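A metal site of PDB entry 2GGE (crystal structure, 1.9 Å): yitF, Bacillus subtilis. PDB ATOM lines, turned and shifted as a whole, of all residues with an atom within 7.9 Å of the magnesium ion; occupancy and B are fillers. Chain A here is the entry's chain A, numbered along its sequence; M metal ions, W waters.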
ATOM      1  N   ASP A  24     -19.743  34.283  -1.389  1.00  0.00           N
ATOM      2  CA  ASP A  24     -19.111  34.457  -2.674  1.00  0.00           C
ATOM      3  C   ASP A  24     -19.825  35.588  -3.503  1.00  0.00           C
ATOM      4  O   ASP A  24     -20.549  36.434  -2.908  1.00  0.00           O
ATOM      5  CB  ASP A  24     -19.140  33.134  -3.441  1.00  0.00           C
ATOM      6  CG  ASP A  24     -20.574  32.566  -3.600  1.00  0.00           C
ATOM      7  OD1 ASP A  24     -21.557  33.351  -3.612  1.00  0.00           O
ATOM      8  OD2 ASP A  24     -20.707  31.337  -3.743  1.00  0.00           O
ATOM      9  N   TYR A 127      -8.305  20.113  -2.832  1.00  0.00           N
ATOM     10  CA  TYR A 127      -7.902  21.482  -2.555  1.00  0.00           C
ATOM     11  C   TYR A 127      -8.827  22.026  -1.495  1.00  0.00           C
ATOM     12  O   TYR A 127     -10.006  21.697  -1.459  1.00  0.00           O
ATOM     13  CB  TYR A 127      -7.867  22.319  -3.846  1.00  0.00           C
ATOM     14  CG  TYR A 127      -9.215  22.382  -4.615  1.00  0.00           C
ATOM     15  CD1 TYR A 127      -9.475  21.556  -5.716  1.00  0.00           C
ATOM     16  CD2 TYR A 127     -10.189  23.296  -4.244  1.00  0.00           C
ATOM     17  CE1 TYR A 127     -10.685  21.627  -6.388  1.00  0.00           C
ATOM     18  CE2 TYR A 127     -11.392  23.403  -4.957  1.00  0.00           C
ATOM     19  CZ  TYR A 127     -11.635  22.557  -6.012  1.00  0.00           C
ATOM     20  OH  TYR A 127     -12.886  22.654  -6.702  1.00  0.00           O
ATOM     21  N   SER A 129     -11.275  24.697  -0.149  1.00  0.00           N
ATOM     22  CA  SER A 129     -12.170  25.557  -0.779  1.00  0.00           C
ATOM     23  C   SER A 129     -12.831  26.517   0.225  1.00  0.00           C
ATOM     24  O   SER A 129     -13.445  26.104   1.247  1.00  0.00           O
ATOM     25  CB  SER A 129     -13.120  24.729  -1.588  1.00  0.00           C
ATOM     26  OG  SER A 129     -13.997  25.539  -2.303  1.00  0.00           O
ATOM     27  N   LYS A 159      -8.904  27.122  -3.395  1.00  0.00           N
ATOM     28  CA  LYS A 159      -9.864  27.812  -4.170  1.00  0.00           C
ATOM     29  C   LYS A 159     -10.416  28.971  -3.356  1.00  0.00           C
ATOM     30  O   LYS A 159     -10.872  28.820  -2.210  1.00  0.00           O
ATOM     31  CB  LYS A 159     -10.989  26.918  -4.677  1.00  0.00           C
ATOM     32  CG  LYS A 159     -11.942  27.629  -5.622  1.00  0.00           C
ATOM     33  CD  LYS A 159     -12.627  26.624  -6.557  1.00  0.00           C
ATOM     34  CE  LYS A 159     -13.949  26.079  -5.822  1.00  0.00           C
ATOM     35  NZ  LYS A 159     -14.674  25.112  -6.630  1.00  0.00           N
ATOM     36  N   LYS A 161     -12.540  33.050  -3.821  1.00  0.00           N
ATOM     37  CA  LYS A 161     -13.631  33.731  -4.520  1.00  0.00           C
ATOM     38  C   LYS A 161     -13.260  35.117  -5.043  1.00  0.00           C
ATOM     39  O   LYS A 161     -12.606  35.910  -4.327  1.00  0.00           O
ATOM     40  CB  LYS A 161     -14.835  33.855  -3.612  1.00  0.00           C
ATOM     41  CG  LYS A 161     -15.345  32.499  -3.020  1.00  0.00           C
ATOM     42  CD  LYS A 161     -15.476  31.363  -4.040  1.00  0.00           C
ATOM     43  CE  LYS A 161     -16.576  30.488  -3.569  1.00  0.00           C
ATOM     44  NZ  LYS A 161     -16.601  29.262  -4.385  1.00  0.00           N
ATOM     45  N   ILE A 188      -6.709  28.598  -7.131  1.00  0.00           N
ATOM     46  CA  ILE A 188      -7.816  28.522  -8.050  1.00  0.00           C
ATOM     47  C   ILE A 188      -8.688  29.737  -7.796  1.00  0.00           C
ATOM     48  O   ILE A 188      -8.940  30.101  -6.644  1.00  0.00           O
ATOM     49  CB  ILE A 188      -8.628  27.228  -7.888  1.00  0.00           C
ATOM     50  CG1 ILE A 188      -7.750  26.026  -8.242  1.00  0.00           C
ATOM     51  CG2 ILE A 188      -9.963  27.349  -8.699  1.00  0.00           C
ATOM     52  CD1 ILE A 188      -8.102  24.787  -7.465  1.00  0.00           C
ATOM     53  N   ASP A 190     -12.321  31.505  -8.328  1.00  0.00           N
ATOM     54  CA  ASP A 190     -13.684  31.193  -8.705  1.00  0.00           C
ATOM     55  C   ASP A 190     -14.553  32.451  -8.717  1.00  0.00           C
ATOM     56  O   ASP A 190     -14.749  33.118  -7.656  1.00  0.00           O
ATOM     57  CB  ASP A 190     -14.225  30.126  -7.699  1.00  0.00           C
ATOM     58  CG  ASP A 190     -15.670  29.746  -7.968  1.00  0.00           C
ATOM     59  OD1 ASP A 190     -16.278  30.119  -9.035  1.00  0.00           O
ATOM     60  OD2 ASP A 190     -16.201  29.055  -7.083  1.00  0.00           O
ATOM     61  N   ALA A 191     -15.136  32.732  -9.887  1.00  0.00           N
ATOM     62  CA  ALA A 191     -15.871  33.942 -10.083  1.00  0.00           C
ATOM     63  C   ALA A 191     -17.348  33.728 -10.050  1.00  0.00           C
ATOM     64  O   ALA A 191     -18.090  34.699 -10.153  1.00  0.00           O
ATOM     65  CB  ALA A 191     -15.463  34.613 -11.363  1.00  0.00           C
ATOM     66  N   ASN A 192     -17.807  32.487  -9.858  1.00  0.00           N
ATOM     67  CA  ASN A 192     -19.281  32.240  -9.707  1.00  0.00           C
ATOM     68  C   ASN A 192     -20.155  32.931 -10.757  1.00  0.00           C
ATOM     69  O   ASN A 192     -21.201  33.569 -10.413  1.00  0.00           O
ATOM     70  CB  ASN A 192     -19.750  32.598  -8.299  1.00  0.00           C
ATOM     71  CG  ASN A 192     -19.191  31.593  -7.221  1.00  0.00           C
ATOM     72  OD1 ASN A 192     -18.210  31.918  -6.518  1.00  0.00           O
ATOM     73  ND2 ASN A 192     -19.711  30.336  -7.215  1.00  0.00           N
ATOM     74  N   GLN A 193     -19.704  32.878 -12.006  1.00  0.00           N
ATOM     75  CA  GLN A 193     -20.373  33.507 -13.159  1.00  0.00           C
ATOM     76  C   GLN A 193     -20.698  35.033 -13.061  1.00  0.00           C
ATOM     77  O   GLN A 193     -21.684  35.505 -13.621  1.00  0.00           O
ATOM     78  CB  GLN A 193     -21.690  32.732 -13.461  1.00  0.00           C
ATOM     79  CG  GLN A 193     -21.564  31.137 -13.326  1.00  0.00           C
ATOM     80  CD  GLN A 193     -22.862  30.361 -13.739  1.00  0.00           C
ATOM     81  OE1 GLN A 193     -23.858  30.943 -14.194  1.00  0.00           O
ATOM     82  NE2 GLN A 193     -22.817  29.057 -13.607  1.00  0.00           N
ATOM     83  N   TRP A 215      -6.678  27.192 -12.070  1.00  0.00           N
ATOM     84  CA  TRP A 215      -7.568  27.562 -13.147  1.00  0.00           C
ATOM     85  C   TRP A 215      -8.476  28.712 -12.735  1.00  0.00           C
ATOM     86  O   TRP A 215      -8.510  29.162 -11.539  1.00  0.00           O
ATOM     87  CB  TRP A 215      -8.413  26.363 -13.574  1.00  0.00           C
ATOM     88  CG  TRP A 215      -9.365  25.809 -12.496  1.00  0.00           C
ATOM     89  CD1 TRP A 215     -10.595  26.317 -12.127  1.00  0.00           C
ATOM     90  CD2 TRP A 215      -9.206  24.591 -11.725  1.00  0.00           C
ATOM     91  NE1 TRP A 215     -11.208  25.497 -11.190  1.00  0.00           N
ATOM     92  CE2 TRP A 215     -10.350  24.465 -10.890  1.00  0.00           C
ATOM     93  CE3 TRP A 215      -8.169  23.670 -11.567  1.00  0.00           C
ATOM     94  CZ2 TRP A 215     -10.508  23.380 -10.025  1.00  0.00           C
ATOM     95  CZ3 TRP A 215      -8.345  22.573 -10.696  1.00  0.00           C
ATOM     96  CH2 TRP A 215      -9.483  22.462  -9.937  1.00  0.00           C
ATOM     97  N   GLU A 217     -12.368  29.517 -12.550  1.00  0.00           N
ATOM     98  CA  GLU A 217     -13.595  28.767 -12.458  1.00  0.00           C
ATOM     99  C   GLU A 217     -14.855  29.567 -12.740  1.00  0.00           C
ATOM    100  O   GLU A 217     -15.120  30.568 -12.088  1.00  0.00           O
ATOM    101  CB  GLU A 217     -13.696  28.086 -11.062  1.00  0.00           C
ATOM    102  CG  GLU A 217     -14.877  27.037 -10.945  1.00  0.00           C
ATOM    103  CD  GLU A 217     -14.748  26.248  -9.660  1.00  0.00           C
ATOM    104  OE1 GLU A 217     -13.636  25.718  -9.371  1.00  0.00           O
ATOM    105  OE2 GLU A 217     -15.731  26.246  -8.878  1.00  0.00           O
ATOM    106  N   GLU A 218     -15.677  29.069 -13.680  1.00  0.00           N
ATOM    107  CA  GLU A 218     -16.952  29.625 -14.138  1.00  0.00           C
ATOM    108  C   GLU A 218     -16.910  31.132 -14.197  1.00  0.00           C
ATOM    109  O   GLU A 218     -17.621  31.796 -13.444  1.00  0.00           O
ATOM    110  CB  GLU A 218     -18.126  29.131 -13.207  1.00  0.00           C
ATOM    111  CG  GLU A 218     -18.306  27.658 -13.342  1.00  0.00           C
ATOM    112  CD  GLU A 218     -19.641  27.114 -12.934  1.00  0.00           C
ATOM    113  OE1 GLU A 218     -20.700  27.810 -12.885  1.00  0.00           O
ATOM    114  OE2 GLU A 218     -19.636  25.903 -12.691  1.00  0.00           O
ATOM    115  N   ALA A 240     -12.365  26.250 -15.906  1.00  0.00           N
ATOM    116  CA  ALA A 240     -13.168  25.136 -15.402  1.00  0.00           C
ATOM    117  C   ALA A 240     -14.632  25.546 -15.215  1.00  0.00           C
ATOM    118  O   ALA A 240     -14.946  26.721 -14.958  1.00  0.00           O
ATOM    119  CB  ALA A 240     -12.610  24.579 -14.024  1.00  0.00           C
ATOM    120  N   GLY A 241     -15.513  24.559 -15.168  1.00  0.00           N
ATOM    121  CA  GLY A 241     -16.896  24.795 -14.914  1.00  0.00           C
ATOM    122  C   GLY A 241     -17.804  23.574 -15.056  1.00  0.00           C
ATOM    123  O   GLY A 241     -17.364  22.447 -15.290  1.00  0.00           O
ATOM    124  N   GLY A 242     -19.090  23.843 -14.892  1.00  0.00           N
ATOM    125  CA  GLY A 242     -20.095  22.883 -15.186  1.00  0.00           C
ATOM    126  C   GLY A 242     -20.763  22.363 -13.901  1.00  0.00           C
ATOM    127  O   GLY A 242     -21.419  21.304 -13.931  1.00  0.00           O
ATOM    128  N   GLU A 243     -20.644  23.124 -12.801  1.00  0.00           N
ATOM    129  CA  GLU A 243     -21.104  22.602 -11.497  1.00  0.00           C
ATOM    130  C   GLU A 243     -22.625  22.361 -11.506  1.00  0.00           C
ATOM    131  O   GLU A 243     -23.135  21.551 -10.731  1.00  0.00           O
ATOM    132  CB  GLU A 243     -20.684  23.511 -10.326  1.00  0.00           C
ATOM    133  CG  GLU A 243     -21.578  24.792 -10.155  1.00  0.00           C
ATOM    134  CD  GLU A 243     -20.988  25.746  -9.050  1.00  0.00           C
ATOM    135  OE1 GLU A 243     -21.726  26.176  -8.109  1.00  0.00           O
ATOM    136  OE2 GLU A 243     -19.755  26.016  -9.090  1.00  0.00           O
ATOM    137  N   ASN A 244     -23.375  23.108 -12.332  1.00  0.00           N
ATOM    138  CA  ASN A 244     -24.820  22.944 -12.316  1.00  0.00           C
ATOM    139  C   ASN A 244     -25.359  22.001 -13.376  1.00  0.00           C
ATOM    140  O   ASN A 244     -26.600  21.882 -13.521  1.00  0.00           O
ATOM    141  CB  ASN A 244     -25.515  24.276 -12.363  1.00  0.00           C
ATOM    142  CG  ASN A 244     -25.262  25.079 -11.117  1.00  0.00           C
ATOM    143  OD1 ASN A 244     -25.376  24.551 -10.011  1.00  0.00           O
ATOM    144  ND2 ASN A 244     -24.851  26.328 -11.276  1.00  0.00           N
ATOM    145  N   GLN A 264     -16.617  19.985 -13.986  1.00  0.00           N
ATOM    146  CA  GLN A 264     -16.746  19.979 -12.538  1.00  0.00           C
ATOM    147  C   GLN A 264     -18.092  19.480 -12.130  1.00  0.00           C
ATOM    148  O   GLN A 264     -18.870  20.199 -11.516  1.00  0.00           O
ATOM    149  CB  GLN A 264     -16.505  21.426 -12.095  1.00  0.00           C
ATOM    150  CG  GLN A 264     -15.015  21.777 -12.127  1.00  0.00           C
ATOM    151  CD  GLN A 264     -14.826  23.066 -11.354  1.00  0.00           C
ATOM    152  OE1 GLN A 264     -15.363  24.064 -11.773  1.00  0.00           O
ATOM    153  NE2 GLN A 264     -14.195  23.022 -10.200  1.00  0.00           N
ATOM    154  N   HIS A 293     -16.940  18.734  -8.018  1.00  0.00           N
ATOM    155  CA  HIS A 293     -17.367  19.863  -7.264  1.00  0.00           C
ATOM    156  C   HIS A 293     -18.102  19.336  -6.031  1.00  0.00           C
ATOM    157  O   HIS A 293     -18.956  18.395  -6.155  1.00  0.00           O
ATOM    158  CB  HIS A 293     -18.400  20.688  -8.099  1.00  0.00           C
ATOM    159  CG  HIS A 293     -18.301  22.160  -7.869  1.00  0.00           C
ATOM    160  ND1 HIS A 293     -19.022  22.813  -6.889  1.00  0.00           N
ATOM    161  CD2 HIS A 293     -17.508  23.102  -8.449  1.00  0.00           C
ATOM    162  CE1 HIS A 293     -18.710  24.097  -6.895  1.00  0.00           C
ATOM    163  NE2 HIS A 293     -17.796  24.307  -7.846  1.00  0.00           N
ATOM    164  N   ALA A 294     -17.912  20.017  -4.888  1.00  0.00           N
ATOM    165  CA  ALA A 294     -18.492  19.524  -3.626  1.00  0.00           C
ATOM    166  C   ALA A 294     -18.509  20.611  -2.610  1.00  0.00           C
ATOM    167  O   ALA A 294     -17.854  20.489  -1.622  1.00  0.00           O
ATOM    168  CB  ALA A 294     -17.669  18.339  -3.101  1.00  0.00           C
ATOM    169  N   TYR A 295     -19.210  21.711  -2.868  1.00  0.00           N
ATOM    170  CA  TYR A 295     -19.411  22.740  -1.882  1.00  0.00           C
ATOM    171  C   TYR A 295     -20.158  22.085  -0.696  1.00  0.00           C
ATOM    172  O   TYR A 295     -19.628  22.078   0.427  1.00  0.00           O
ATOM    173  CB  TYR A 295     -20.230  23.891  -2.459  1.00  0.00           C
ATOM    174  CG  TYR A 295     -20.666  24.904  -1.396  1.00  0.00           C
ATOM    175  CD1 TYR A 295     -22.050  25.229  -1.212  1.00  0.00           C
ATOM    176  CD2 TYR A 295     -19.712  25.481  -0.546  1.00  0.00           C
ATOM    177  CE1 TYR A 295     -22.460  26.157  -0.179  1.00  0.00           C
ATOM    178  CE2 TYR A 295     -20.083  26.405   0.474  1.00  0.00           C
ATOM    179  CZ  TYR A 295     -21.452  26.746   0.637  1.00  0.00           C
ATOM    180  OH  TYR A 295     -21.814  27.666   1.637  1.00  0.00           O
ATOM    181  N   GLU A 326     -12.781  18.944  -4.733  1.00  0.00           N
ATOM    182  CA  GLU A 326     -13.016  20.062  -3.865  1.00  0.00           C
ATOM    183  C   GLU A 326     -13.267  19.645  -2.391  1.00  0.00           C
ATOM    184  O   GLU A 326     -14.088  18.708  -2.081  1.00  0.00           O
ATOM    185  CB  GLU A 326     -14.193  20.874  -4.431  1.00  0.00           C
ATOM    186  CG  GLU A 326     -14.719  21.893  -3.462  1.00  0.00           C
ATOM    187  CD  GLU A 326     -15.670  22.911  -4.101  1.00  0.00           C
ATOM    188  OE1 GLU A 326     -16.554  22.486  -4.894  1.00  0.00           O
ATOM    189  OE2 GLU A 326     -15.605  24.106  -3.717  1.00  0.00           O
HETATM  190 MG    MG M   1     -17.702  26.299  -8.929  1.00  0.00          MG
HETATM  191  O   HOH W   1     -17.808  27.067  -6.910  1.00  0.00           O
HETATM  192  O   HOH W   2     -18.092  28.285  -9.791  1.00  0.00           O
HETATM  193  O   HOH W   3     -17.841  25.159 -10.906  1.00  0.00           O
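The side-chain carboxylate (OE1) of Glu 217 is in salt-bridge range of the side-chain amino group (NZ) of Lys 159 (3.0 Å).
NE2 of Gln 264 sits at hydrogen-bond distance from OE1 of Glu 217, 2.9 Å away.
NE1 of Trp 215 lies within hydrogen-bond range of OE1 of Glu 217.
The backbone NH (N) of Ala 191 is in hydrogen-bond range of the backbone carbonyl oxygen (O) of Glu 217 (3.1 Å).
The side-chain carboxylate (OE2) of Glu 218 sits at hydrogen-bond distance from the backbone NH (N) of Glu 243 (3.0 Å).
The side-chain amino group (NZ) of Lys 161 lies within salt-bridge range of the side-chain carboxylate (OD2) of Asp 190 (2.7 Å).
OE2 of Glu 326 is in salt-bridge range of NZ of Lys 159 (3.2 Å).
The side-chain amino group (NZ) of Lys 159 lies within hydrogen-bond range of the side-chain hydroxyl (OH) of Tyr 127 (3.0 Å).
NZ of Lys 159 touches the magnesium ion, 3.98 Å away.
Asp 190 touches the magnesium ion (OD2 to MG, 3.6 Å).
The magnesium ion is bound by OE2 of Glu 217 (2.0 Å).
The magnesium ion is bound by OE2 of Glu 243.
Water W1 is bound to the magnesium ion (2.2 Å).
The magnesium ion is bound by water W2.
A ring nitrogen (NE2) of His 293 binds the magnesium ion, 2.3 Å away.
The magnesium ion is bound by water W3, at 2.3 Å.
Water W3 lies within hydrogen-bond range of the side-chain carboxylate of Glu 218 (2.6 Å) and the side-chain amide oxygen of Gln 264 (2.8 Å).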
